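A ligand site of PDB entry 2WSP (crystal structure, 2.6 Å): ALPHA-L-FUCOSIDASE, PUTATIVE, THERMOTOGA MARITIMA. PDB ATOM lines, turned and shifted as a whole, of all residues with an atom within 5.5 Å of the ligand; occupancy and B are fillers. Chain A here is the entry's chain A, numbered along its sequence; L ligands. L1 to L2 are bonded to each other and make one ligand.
OE1 of Glu 66 is in hydrogen-bond range of O2 of LG2 L2 (2.5 Å).
NE2 of His 34 is in hydrogen-bond range of O3 of LG2 L2 (2.6 Å).
A ring nitrogen (NE2) of His 128 sits at hydrogen-bond distance from an oxygen (O2) of LG2 L2, at 2.9 Å.
A ring nitrogen (NE2) of His 129 sits at hydrogen-bond distance from an oxygen (O1) of LG2 L2 (2.9 Å).
An oxygen (O1) of LG2 L2 lies within hydrogen-bond range of the indole nitrogen (NE1) of Trp 67 (3.1 Å).
The backbone NH of Phe 290 is in hydrogen-bond range of the side-chain carboxylate of Glu 66, 3.4 Å away.
The backbone NH (N) of Tyr 64 is in hydrogen-bond range of the side-chain amide oxygen (OD1) of Asn 62.
CE2 of Phe 32 touches C6 of LG2 L2, 3.9 Å away.
NE1 of Trp 58 touches N3 of LIG L1 (3.8 Å).
Tyr 64 touches the ligand.
OH of Tyr 171 touches O3 of LG2 L2, at 3.8 Å.
NH1 of Arg 254 touches O2 of LIG L1 (3.6 Å).
CG of Glu 266 touches O2 of LIG L1, at 3.2 Å.
CE2 of Phe 290 touches C6 of LG2 L2, 3.4 Å away.
Of the 19 residues printed, 12 come within 4 Å of the ligand.
The nearest printed residue that does not touch the ligand is Leu 50 (4.2 Å).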
ATOM      1  N   PHE A  32     -14.376  -3.583  -2.062  1.00  0.00           N
ATOM      2  CA  PHE A  32     -12.934  -3.528  -1.872  1.00  0.00           C
ATOM      3  C   PHE A  32     -12.728  -3.025  -0.442  1.00  0.00           C
ATOM      4  O   PHE A  32     -13.496  -2.177   0.007  1.00  0.00           O
ATOM      5  CB  PHE A  32     -12.354  -2.500  -2.860  1.00  0.00           C
ATOM      6  CG  PHE A  32     -11.043  -2.883  -3.502  1.00  0.00           C
ATOM      7  CD1 PHE A  32     -10.167  -3.799  -2.945  1.00  0.00           C
ATOM      8  CD2 PHE A  32     -10.664  -2.259  -4.688  1.00  0.00           C
ATOM      9  CE1 PHE A  32      -8.959  -4.104  -3.572  1.00  0.00           C
ATOM     10  CE2 PHE A  32      -9.470  -2.566  -5.315  1.00  0.00           C
ATOM     11  CZ  PHE A  32      -8.622  -3.486  -4.757  1.00  0.00           C
ATOM     12  N   HIS A  34      -9.549  -1.297   1.669  1.00  0.00           N
ATOM     13  CA  HIS A  34      -8.195  -0.848   1.957  1.00  0.00           C
ATOM     14  C   HIS A  34      -8.101  -0.498   3.430  1.00  0.00           C
ATOM     15  O   HIS A  34      -8.590   0.540   3.871  1.00  0.00           O
ATOM     16  CB  HIS A  34      -7.814   0.356   1.099  1.00  0.00           C
ATOM     17  CG  HIS A  34      -7.461  -0.004  -0.309  1.00  0.00           C
ATOM     18  ND1 HIS A  34      -8.382  -0.524  -1.194  1.00  0.00           N
ATOM     19  CD2 HIS A  34      -6.296   0.085  -0.990  1.00  0.00           C
ATOM     20  CE1 HIS A  34      -7.800  -0.729  -2.358  1.00  0.00           C
ATOM     21  NE2 HIS A  34      -6.533  -0.367  -2.269  1.00  0.00           N
ATOM     22  N   LEU A  50      -8.072  10.758 -10.604  1.00  0.00           N
ATOM     23  CA  LEU A  50      -7.180  10.547 -11.739  1.00  0.00           C
ATOM     24  C   LEU A  50      -7.735  11.249 -12.981  1.00  0.00           C
ATOM     25  O   LEU A  50      -8.918  11.096 -13.311  1.00  0.00           O
ATOM     26  CB  LEU A  50      -6.993   9.050 -12.025  1.00  0.00           C
ATOM     27  CG  LEU A  50      -6.077   8.247 -11.088  1.00  0.00           C
ATOM     28  CD1 LEU A  50      -6.442   6.769 -11.124  1.00  0.00           C
ATOM     29  CD2 LEU A  50      -4.603   8.460 -11.418  1.00  0.00           C
ATOM     30  N   MET A  55      -0.802  15.080 -12.827  1.00  0.00           N
ATOM     31  CA  MET A  55      -0.010  13.913 -12.430  1.00  0.00           C
ATOM     32  C   MET A  55       1.446  14.260 -12.077  1.00  0.00           C
ATOM     33  O   MET A  55       2.189  13.419 -11.554  1.00  0.00           O
ATOM     34  CB  MET A  55      -0.034  12.851 -13.544  1.00  0.00           C
ATOM     35  CG  MET A  55       0.170  11.414 -13.060  1.00  0.00           C
ATOM     36  SD  MET A  55      -1.252  10.770 -12.147  1.00  0.00           S
ATOM     37  CE  MET A  55      -0.644   9.167 -11.609  1.00  0.00           C
ATOM     38  N   TRP A  58       0.881  14.863  -8.306  1.00  0.00           N
ATOM     39  CA  TRP A  58       0.063  13.822  -7.660  1.00  0.00           C
ATOM     40  C   TRP A  58       0.706  13.204  -6.421  1.00  0.00           C
ATOM     41  O   TRP A  58       0.075  13.119  -5.379  1.00  0.00           O
ATOM     42  CB  TRP A  58      -0.282  12.728  -8.673  1.00  0.00           C
ATOM     43  CG  TRP A  58      -1.088  11.591  -8.099  1.00  0.00           C
ATOM     44  CD1 TRP A  58      -0.615  10.454  -7.511  1.00  0.00           C
ATOM     45  CD2 TRP A  58      -2.522  11.482  -8.060  1.00  0.00           C
ATOM     46  NE1 TRP A  58      -1.653   9.651  -7.104  1.00  0.00           N
ATOM     47  CE2 TRP A  58      -2.837  10.263  -7.434  1.00  0.00           C
ATOM     48  CE3 TRP A  58      -3.574  12.307  -8.492  1.00  0.00           C
ATOM     49  CZ2 TRP A  58      -4.155   9.832  -7.233  1.00  0.00           C
ATOM     50  CZ3 TRP A  58      -4.881  11.892  -8.291  1.00  0.00           C
ATOM     51  CH2 TRP A  58      -5.165  10.662  -7.666  1.00  0.00           C
ATOM     52  N   PHE A  59       1.958  12.761  -6.541  1.00  0.00           N
ATOM     53  CA  PHE A  59       2.620  12.076  -5.443  1.00  0.00           C
ATOM     54  C   PHE A  59       3.016  13.033  -4.323  1.00  0.00           C
ATOM     55  O   PHE A  59       3.134  12.621  -3.162  1.00  0.00           O
ATOM     56  CB  PHE A  59       3.841  11.299  -5.937  1.00  0.00           C
ATOM     57  CG  PHE A  59       3.495  10.219  -6.929  1.00  0.00           C
ATOM     58  CD1 PHE A  59       2.897   9.035  -6.503  1.00  0.00           C
ATOM     59  CD2 PHE A  59       3.726  10.390  -8.286  1.00  0.00           C
ATOM     60  CE1 PHE A  59       2.557   8.040  -7.415  1.00  0.00           C
ATOM     61  CE2 PHE A  59       3.391   9.403  -9.198  1.00  0.00           C
ATOM     62  CZ  PHE A  59       2.813   8.229  -8.763  1.00  0.00           C
ATOM     63  N   ASN A  62      -0.663  13.700  -2.593  1.00  0.00           N
ATOM     64  CA  ASN A  62      -1.353  12.438  -2.875  1.00  0.00           C
ATOM     65  C   ASN A  62      -2.678  12.282  -2.149  1.00  0.00           C
ATOM     66  O   ASN A  62      -2.714  12.276  -0.917  1.00  0.00           O
ATOM     67  CB  ASN A  62      -0.433  11.261  -2.543  1.00  0.00           C
ATOM     68  CG  ASN A  62      -0.814   9.985  -3.287  1.00  0.00           C
ATOM     69  OD1 ASN A  62      -1.987   9.726  -3.548  1.00  0.00           O
ATOM     70  ND2 ASN A  62       0.186   9.189  -3.633  1.00  0.00           N
ATOM     71  N   TYR A  64      -4.492   9.605  -2.070  1.00  0.00           N
ATOM     72  CA  TYR A  64      -4.646   8.225  -1.592  1.00  0.00           C
ATOM     73  C   TYR A  64      -3.962   8.104  -0.237  1.00  0.00           C
ATOM     74  O   TYR A  64      -2.746   8.215  -0.139  1.00  0.00           O
ATOM     75  CB  TYR A  64      -4.022   7.253  -2.598  1.00  0.00           C
ATOM     76  CG  TYR A  64      -4.758   7.088  -3.915  1.00  0.00           C
ATOM     77  CD1 TYR A  64      -4.343   6.149  -4.853  1.00  0.00           C
ATOM     78  CD2 TYR A  64      -5.872   7.873  -4.245  1.00  0.00           C
ATOM     79  CE1 TYR A  64      -4.991   5.995  -6.073  1.00  0.00           C
ATOM     80  CE2 TYR A  64      -6.528   7.725  -5.455  1.00  0.00           C
ATOM     81  CZ  TYR A  64      -6.090   6.781  -6.363  1.00  0.00           C
ATOM     82  OH  TYR A  64      -6.730   6.621  -7.574  1.00  0.00           O
ATOM     83  N   GLU A  66      -3.613   5.575   1.699  1.00  0.00           N
ATOM     84  CA  GLU A  66      -2.774   4.369   1.833  1.00  0.00           C
ATOM     85  C   GLU A  66      -1.320   4.658   1.445  1.00  0.00           C
ATOM     86  O   GLU A  66      -0.425   3.927   1.854  1.00  0.00           O
ATOM     87  CB  GLU A  66      -3.265   3.188   0.984  1.00  0.00           C
ATOM     88  CG  GLU A  66      -4.684   3.248   0.475  1.00  0.00           C
ATOM     89  CD  GLU A  66      -4.811   4.103  -0.780  1.00  0.00           C
ATOM     90  OE1 GLU A  66      -4.412   3.650  -1.861  1.00  0.00           O
ATOM     91  OE2 GLU A  66      -5.329   5.221  -0.667  1.00  0.00           O
ATOM     92  N   TRP A  67      -1.107   5.689   0.630  1.00  0.00           N
ATOM     93  CA  TRP A  67       0.235   6.112   0.228  1.00  0.00           C
ATOM     94  C   TRP A  67       0.980   6.955   1.273  1.00  0.00           C
ATOM     95  O   TRP A  67       2.082   7.435   1.000  1.00  0.00           O
ATOM     96  CB  TRP A  67       0.163   6.862  -1.111  1.00  0.00           C
ATOM     97  CG  TRP A  67       0.028   5.921  -2.259  1.00  0.00           C
ATOM     98  CD1 TRP A  67      -1.049   5.126  -2.542  1.00  0.00           C
ATOM     99  CD2 TRP A  67       1.013   5.642  -3.249  1.00  0.00           C
ATOM    100  NE1 TRP A  67      -0.788   4.376  -3.651  1.00  0.00           N
ATOM    101  CE2 TRP A  67       0.472   4.660  -4.103  1.00  0.00           C
ATOM    102  CE3 TRP A  67       2.309   6.113  -3.499  1.00  0.00           C
ATOM    103  CZ2 TRP A  67       1.176   4.164  -5.205  1.00  0.00           C
ATOM    104  CZ3 TRP A  67       3.000   5.616  -4.590  1.00  0.00           C
ATOM    105  CH2 TRP A  67       2.435   4.652  -5.434  1.00  0.00           C
ATOM    106  N   HIS A 128      -0.615  -4.239   1.343  1.00  0.00           N
ATOM    107  CA  HIS A 128      -0.544  -3.141   0.404  1.00  0.00           C
ATOM    108  C   HIS A 128       0.928  -2.738   0.187  1.00  0.00           C
ATOM    109  O   HIS A 128       1.841  -3.522   0.484  1.00  0.00           O
ATOM    110  CB  HIS A 128      -1.392  -1.969   0.920  1.00  0.00           C
ATOM    111  CG  HIS A 128      -1.864  -1.052  -0.162  1.00  0.00           C
ATOM    112  ND1 HIS A 128      -1.303   0.188  -0.376  1.00  0.00           N
ATOM    113  CD2 HIS A 128      -2.802  -1.222  -1.132  1.00  0.00           C
ATOM    114  CE1 HIS A 128      -1.881   0.747  -1.419  1.00  0.00           C
ATOM    115  NE2 HIS A 128      -2.802  -0.080  -1.887  1.00  0.00           N
ATOM    116  N   HIS A 129       1.171  -1.551  -0.357  1.00  0.00           N
ATOM    117  CA  HIS A 129       2.506  -1.122  -0.719  1.00  0.00           C
ATOM    118  C   HIS A 129       3.450  -0.990   0.480  1.00  0.00           C
ATOM    119  O   HIS A 129       4.648  -1.256   0.354  1.00  0.00           O
ATOM    120  CB  HIS A 129       2.473   0.194  -1.501  1.00  0.00           C
ATOM    121  CG  HIS A 129       1.535   0.184  -2.678  1.00  0.00           C
ATOM    122  ND1 HIS A 129       1.205  -0.978  -3.342  1.00  0.00           N
ATOM    123  CD2 HIS A 129       0.881   1.182  -3.302  1.00  0.00           C
ATOM    124  CE1 HIS A 129       0.373  -0.691  -4.330  1.00  0.00           C
ATOM    125  NE2 HIS A 129       0.160   0.621  -4.325  1.00  0.00           N
ATOM    126  N   TYR A 171      -6.702  -9.065  -2.037  1.00  0.00           N
ATOM    127  CA  TYR A 171      -5.808  -8.107  -2.676  1.00  0.00           C
ATOM    128  C   TYR A 171      -4.390  -8.304  -2.129  1.00  0.00           C
ATOM    129  O   TYR A 171      -4.197  -8.370  -0.916  1.00  0.00           O
ATOM    130  CB  TYR A 171      -6.253  -6.667  -2.431  1.00  0.00           C
ATOM    131  CG  TYR A 171      -5.241  -5.645  -2.924  1.00  0.00           C
ATOM    132  CD1 TYR A 171      -4.126  -5.310  -2.159  1.00  0.00           C
ATOM    133  CD2 TYR A 171      -5.380  -5.056  -4.173  1.00  0.00           C
ATOM    134  CE1 TYR A 171      -3.190  -4.406  -2.621  1.00  0.00           C
ATOM    135  CE2 TYR A 171      -4.446  -4.138  -4.644  1.00  0.00           C
ATOM    136  CZ  TYR A 171      -3.357  -3.822  -3.858  1.00  0.00           C
ATOM    137  OH  TYR A 171      -2.414  -2.910  -4.300  1.00  0.00           O
ATOM    138  N   TRP A 222      -6.427 -10.736  -6.572  1.00  0.00           N
ATOM    139  CA  TRP A 222      -6.409  -9.367  -7.105  1.00  0.00           C
ATOM    140  C   TRP A 222      -5.050  -8.747  -6.815  1.00  0.00           C
ATOM    141  O   TRP A 222      -4.782  -8.308  -5.708  1.00  0.00           O
ATOM    142  CB  TRP A 222      -7.510  -8.541  -6.424  1.00  0.00           C
ATOM    143  CG  TRP A 222      -8.141  -7.451  -7.258  1.00  0.00           C
ATOM    144  CD1 TRP A 222      -9.401  -7.460  -7.804  1.00  0.00           C
ATOM    145  CD2 TRP A 222      -7.574  -6.180  -7.602  1.00  0.00           C
ATOM    146  NE1 TRP A 222      -9.633  -6.281  -8.471  1.00  0.00           N
ATOM    147  CE2 TRP A 222      -8.534  -5.479  -8.359  1.00  0.00           C
ATOM    148  CE3 TRP A 222      -6.337  -5.568  -7.338  1.00  0.00           C
ATOM    149  CZ2 TRP A 222      -8.303  -4.195  -8.861  1.00  0.00           C
ATOM    150  CZ3 TRP A 222      -6.106  -4.284  -7.839  1.00  0.00           C
ATOM    151  CH2 TRP A 222      -7.090  -3.616  -8.596  1.00  0.00           C
ATOM    152  N   MET A 225      -0.155  -3.337  -8.989  1.00  0.00           N
ATOM    153  CA  MET A 225       1.112  -2.745  -9.417  1.00  0.00           C
ATOM    154  C   MET A 225       2.053  -3.714 -10.143  1.00  0.00           C
ATOM    155  O   MET A 225       3.279  -3.536 -10.125  1.00  0.00           O
ATOM    156  CB  MET A 225       1.823  -2.074  -8.222  1.00  0.00           C
ATOM    157  CG  MET A 225       1.084  -0.859  -7.690  1.00  0.00           C
ATOM    158  SD  MET A 225       1.087   0.512  -8.873  1.00  0.00           S
ATOM    159  CE  MET A 225       2.847   0.812  -9.041  1.00  0.00           C
ATOM    160  N   ARG A 254      -3.481  -7.391 -13.517  1.00  0.00           N
ATOM    161  CA  ARG A 254      -2.424  -6.480 -13.113  1.00  0.00           C
ATOM    162  C   ARG A 254      -1.186  -7.243 -12.656  1.00  0.00           C
ATOM    163  O   ARG A 254      -0.517  -6.845 -11.704  1.00  0.00           O
ATOM    164  CB  ARG A 254      -2.942  -5.573 -12.002  1.00  0.00           C
ATOM    165  CG  ARG A 254      -4.141  -4.726 -12.428  1.00  0.00           C
ATOM    166  CD  ARG A 254      -4.396  -3.630 -11.404  1.00  0.00           C
ATOM    167  NE  ARG A 254      -5.553  -2.800 -11.762  1.00  0.00           N
ATOM    168  CZ  ARG A 254      -5.819  -1.604 -11.247  1.00  0.00           C
ATOM    169  NH1 ARG A 254      -5.022  -1.052 -10.327  1.00  0.00           N
ATOM    170  NH2 ARG A 254      -6.896  -0.948 -11.640  1.00  0.00           N
ATOM    171  N   GLU A 266      -9.773   1.916 -13.822  1.00  0.00           N
ATOM    172  CA  GLU A 266      -9.799   2.915 -12.767  1.00  0.00           C
ATOM    173  C   GLU A 266     -10.016   4.323 -13.331  1.00  0.00           C
ATOM    174  O   GLU A 266      -9.587   5.322 -12.743  1.00  0.00           O
ATOM    175  CB  GLU A 266      -8.531   2.798 -11.893  1.00  0.00           C
ATOM    176  CG  GLU A 266      -7.277   2.244 -12.605  1.00  0.00           C
ATOM    177  CD  GLU A 266      -6.587   3.264 -13.507  1.00  0.00           C
ATOM    178  OE1 GLU A 266      -6.110   2.865 -14.600  1.00  0.00           O
ATOM    179  OE2 GLU A 266      -6.498   4.455 -13.124  1.00  0.00           O
ATOM    180  N   THR A 283     -13.186  -0.150 -10.525  1.00  0.00           N
ATOM    181  CA  THR A 283     -12.895   0.001  -9.102  1.00  0.00           C
ATOM    182  C   THR A 283     -12.758   1.492  -8.768  1.00  0.00           C
ATOM    183  O   THR A 283     -12.108   2.232  -9.491  1.00  0.00           O
ATOM    184  CB  THR A 283     -11.610  -0.762  -8.708  1.00  0.00           C
ATOM    185  OG1 THR A 283     -11.507  -0.845  -7.282  1.00  0.00           O
ATOM    186  CG2 THR A 283     -10.358  -0.098  -9.264  1.00  0.00           C
ATOM    187  N   PHE A 290      -8.640   5.454  -1.267  1.00  0.00           N
ATOM    188  CA  PHE A 290      -9.052   4.091  -0.960  1.00  0.00           C
ATOM    189  C   PHE A 290      -8.967   3.847   0.545  1.00  0.00           C
ATOM    190  O   PHE A 290      -9.900   3.306   1.132  1.00  0.00           O
ATOM    191  CB  PHE A 290      -8.192   3.082  -1.714  1.00  0.00           C
ATOM    192  CG  PHE A 290      -8.441   3.074  -3.196  1.00  0.00           C
ATOM    193  CD1 PHE A 290      -7.812   3.991  -4.017  1.00  0.00           C
ATOM    194  CD2 PHE A 290      -9.310   2.156  -3.768  1.00  0.00           C
ATOM    195  CE1 PHE A 290      -8.037   3.992  -5.390  1.00  0.00           C
ATOM    196  CE2 PHE A 290      -9.549   2.154  -5.140  1.00  0.00           C
ATOM    197  CZ  PHE A 290      -8.906   3.073  -5.952  1.00  0.00           C
HETATM  198  C1  LIG L   1      -2.166   4.101  -9.020  1.00  0.00           C
HETATM  199  N1  LIG L   1      -1.314   4.013  -7.831  1.00  0.00           N
HETATM  200  C2  LIG L   1      -3.209   2.984  -9.008  1.00  0.00           C
HETATM  201  N2  LIG L   1      -1.293   4.973  -7.028  1.00  0.00           N
HETATM  202  O1  LIG L   1      -3.796   2.743  -7.729  1.00  0.00           O
HETATM  203  C3  LIG L   1      -4.253   3.406 -10.036  1.00  0.00           C
HETATM  204  N3  LIG L   1      -1.320   5.955  -6.264  1.00  0.00           N
HETATM  205  O2  LIG L   1      -5.352   2.481 -10.039  1.00  0.00           O
HETATM  206  C4  LIG L   1      -3.576   3.490 -11.410  1.00  0.00           C
HETATM  207  O3  LIG L   1      -3.336   2.176 -11.906  1.00  0.00           O
HETATM  208  C5  LIG L   1      -2.240   4.262 -11.387  1.00  0.00           C
HETATM  209  O4  LIG L   1      -1.436   3.947 -10.239  1.00  0.00           O
HETATM  210  C6  LIG L   1      -1.442   3.969 -12.660  1.00  0.00           C
HETATM  211  C1  LG2 L   2      -3.524   1.443  -7.185  1.00  0.00           C
HETATM  212  C2  LG2 L   2      -2.866   1.567  -5.806  1.00  0.00           C
HETATM  213  C3  LG2 L   2      -3.834   2.185  -4.823  1.00  0.00           C
HETATM  214  C4  LG2 L   2      -5.116   1.361  -4.748  1.00  0.00           C
HETATM  215  C5  LG2 L   2      -5.703   1.183  -6.151  1.00  0.00           C
HETATM  216  C6  LG2 L   2      -6.890   0.238  -6.101  1.00  0.00           C
HETATM  217  O1  LG2 L   2      -1.669   2.342  -5.848  1.00  0.00           O
HETATM  218  O2  LG2 L   2      -3.214   2.248  -3.543  1.00  0.00           O
HETATM  219  O3  LG2 L   2      -4.825   0.085  -4.175  1.00  0.00           O
HETATM  220  O4  LG2 L   2      -4.734   0.678  -7.072  1.00  0.00           O
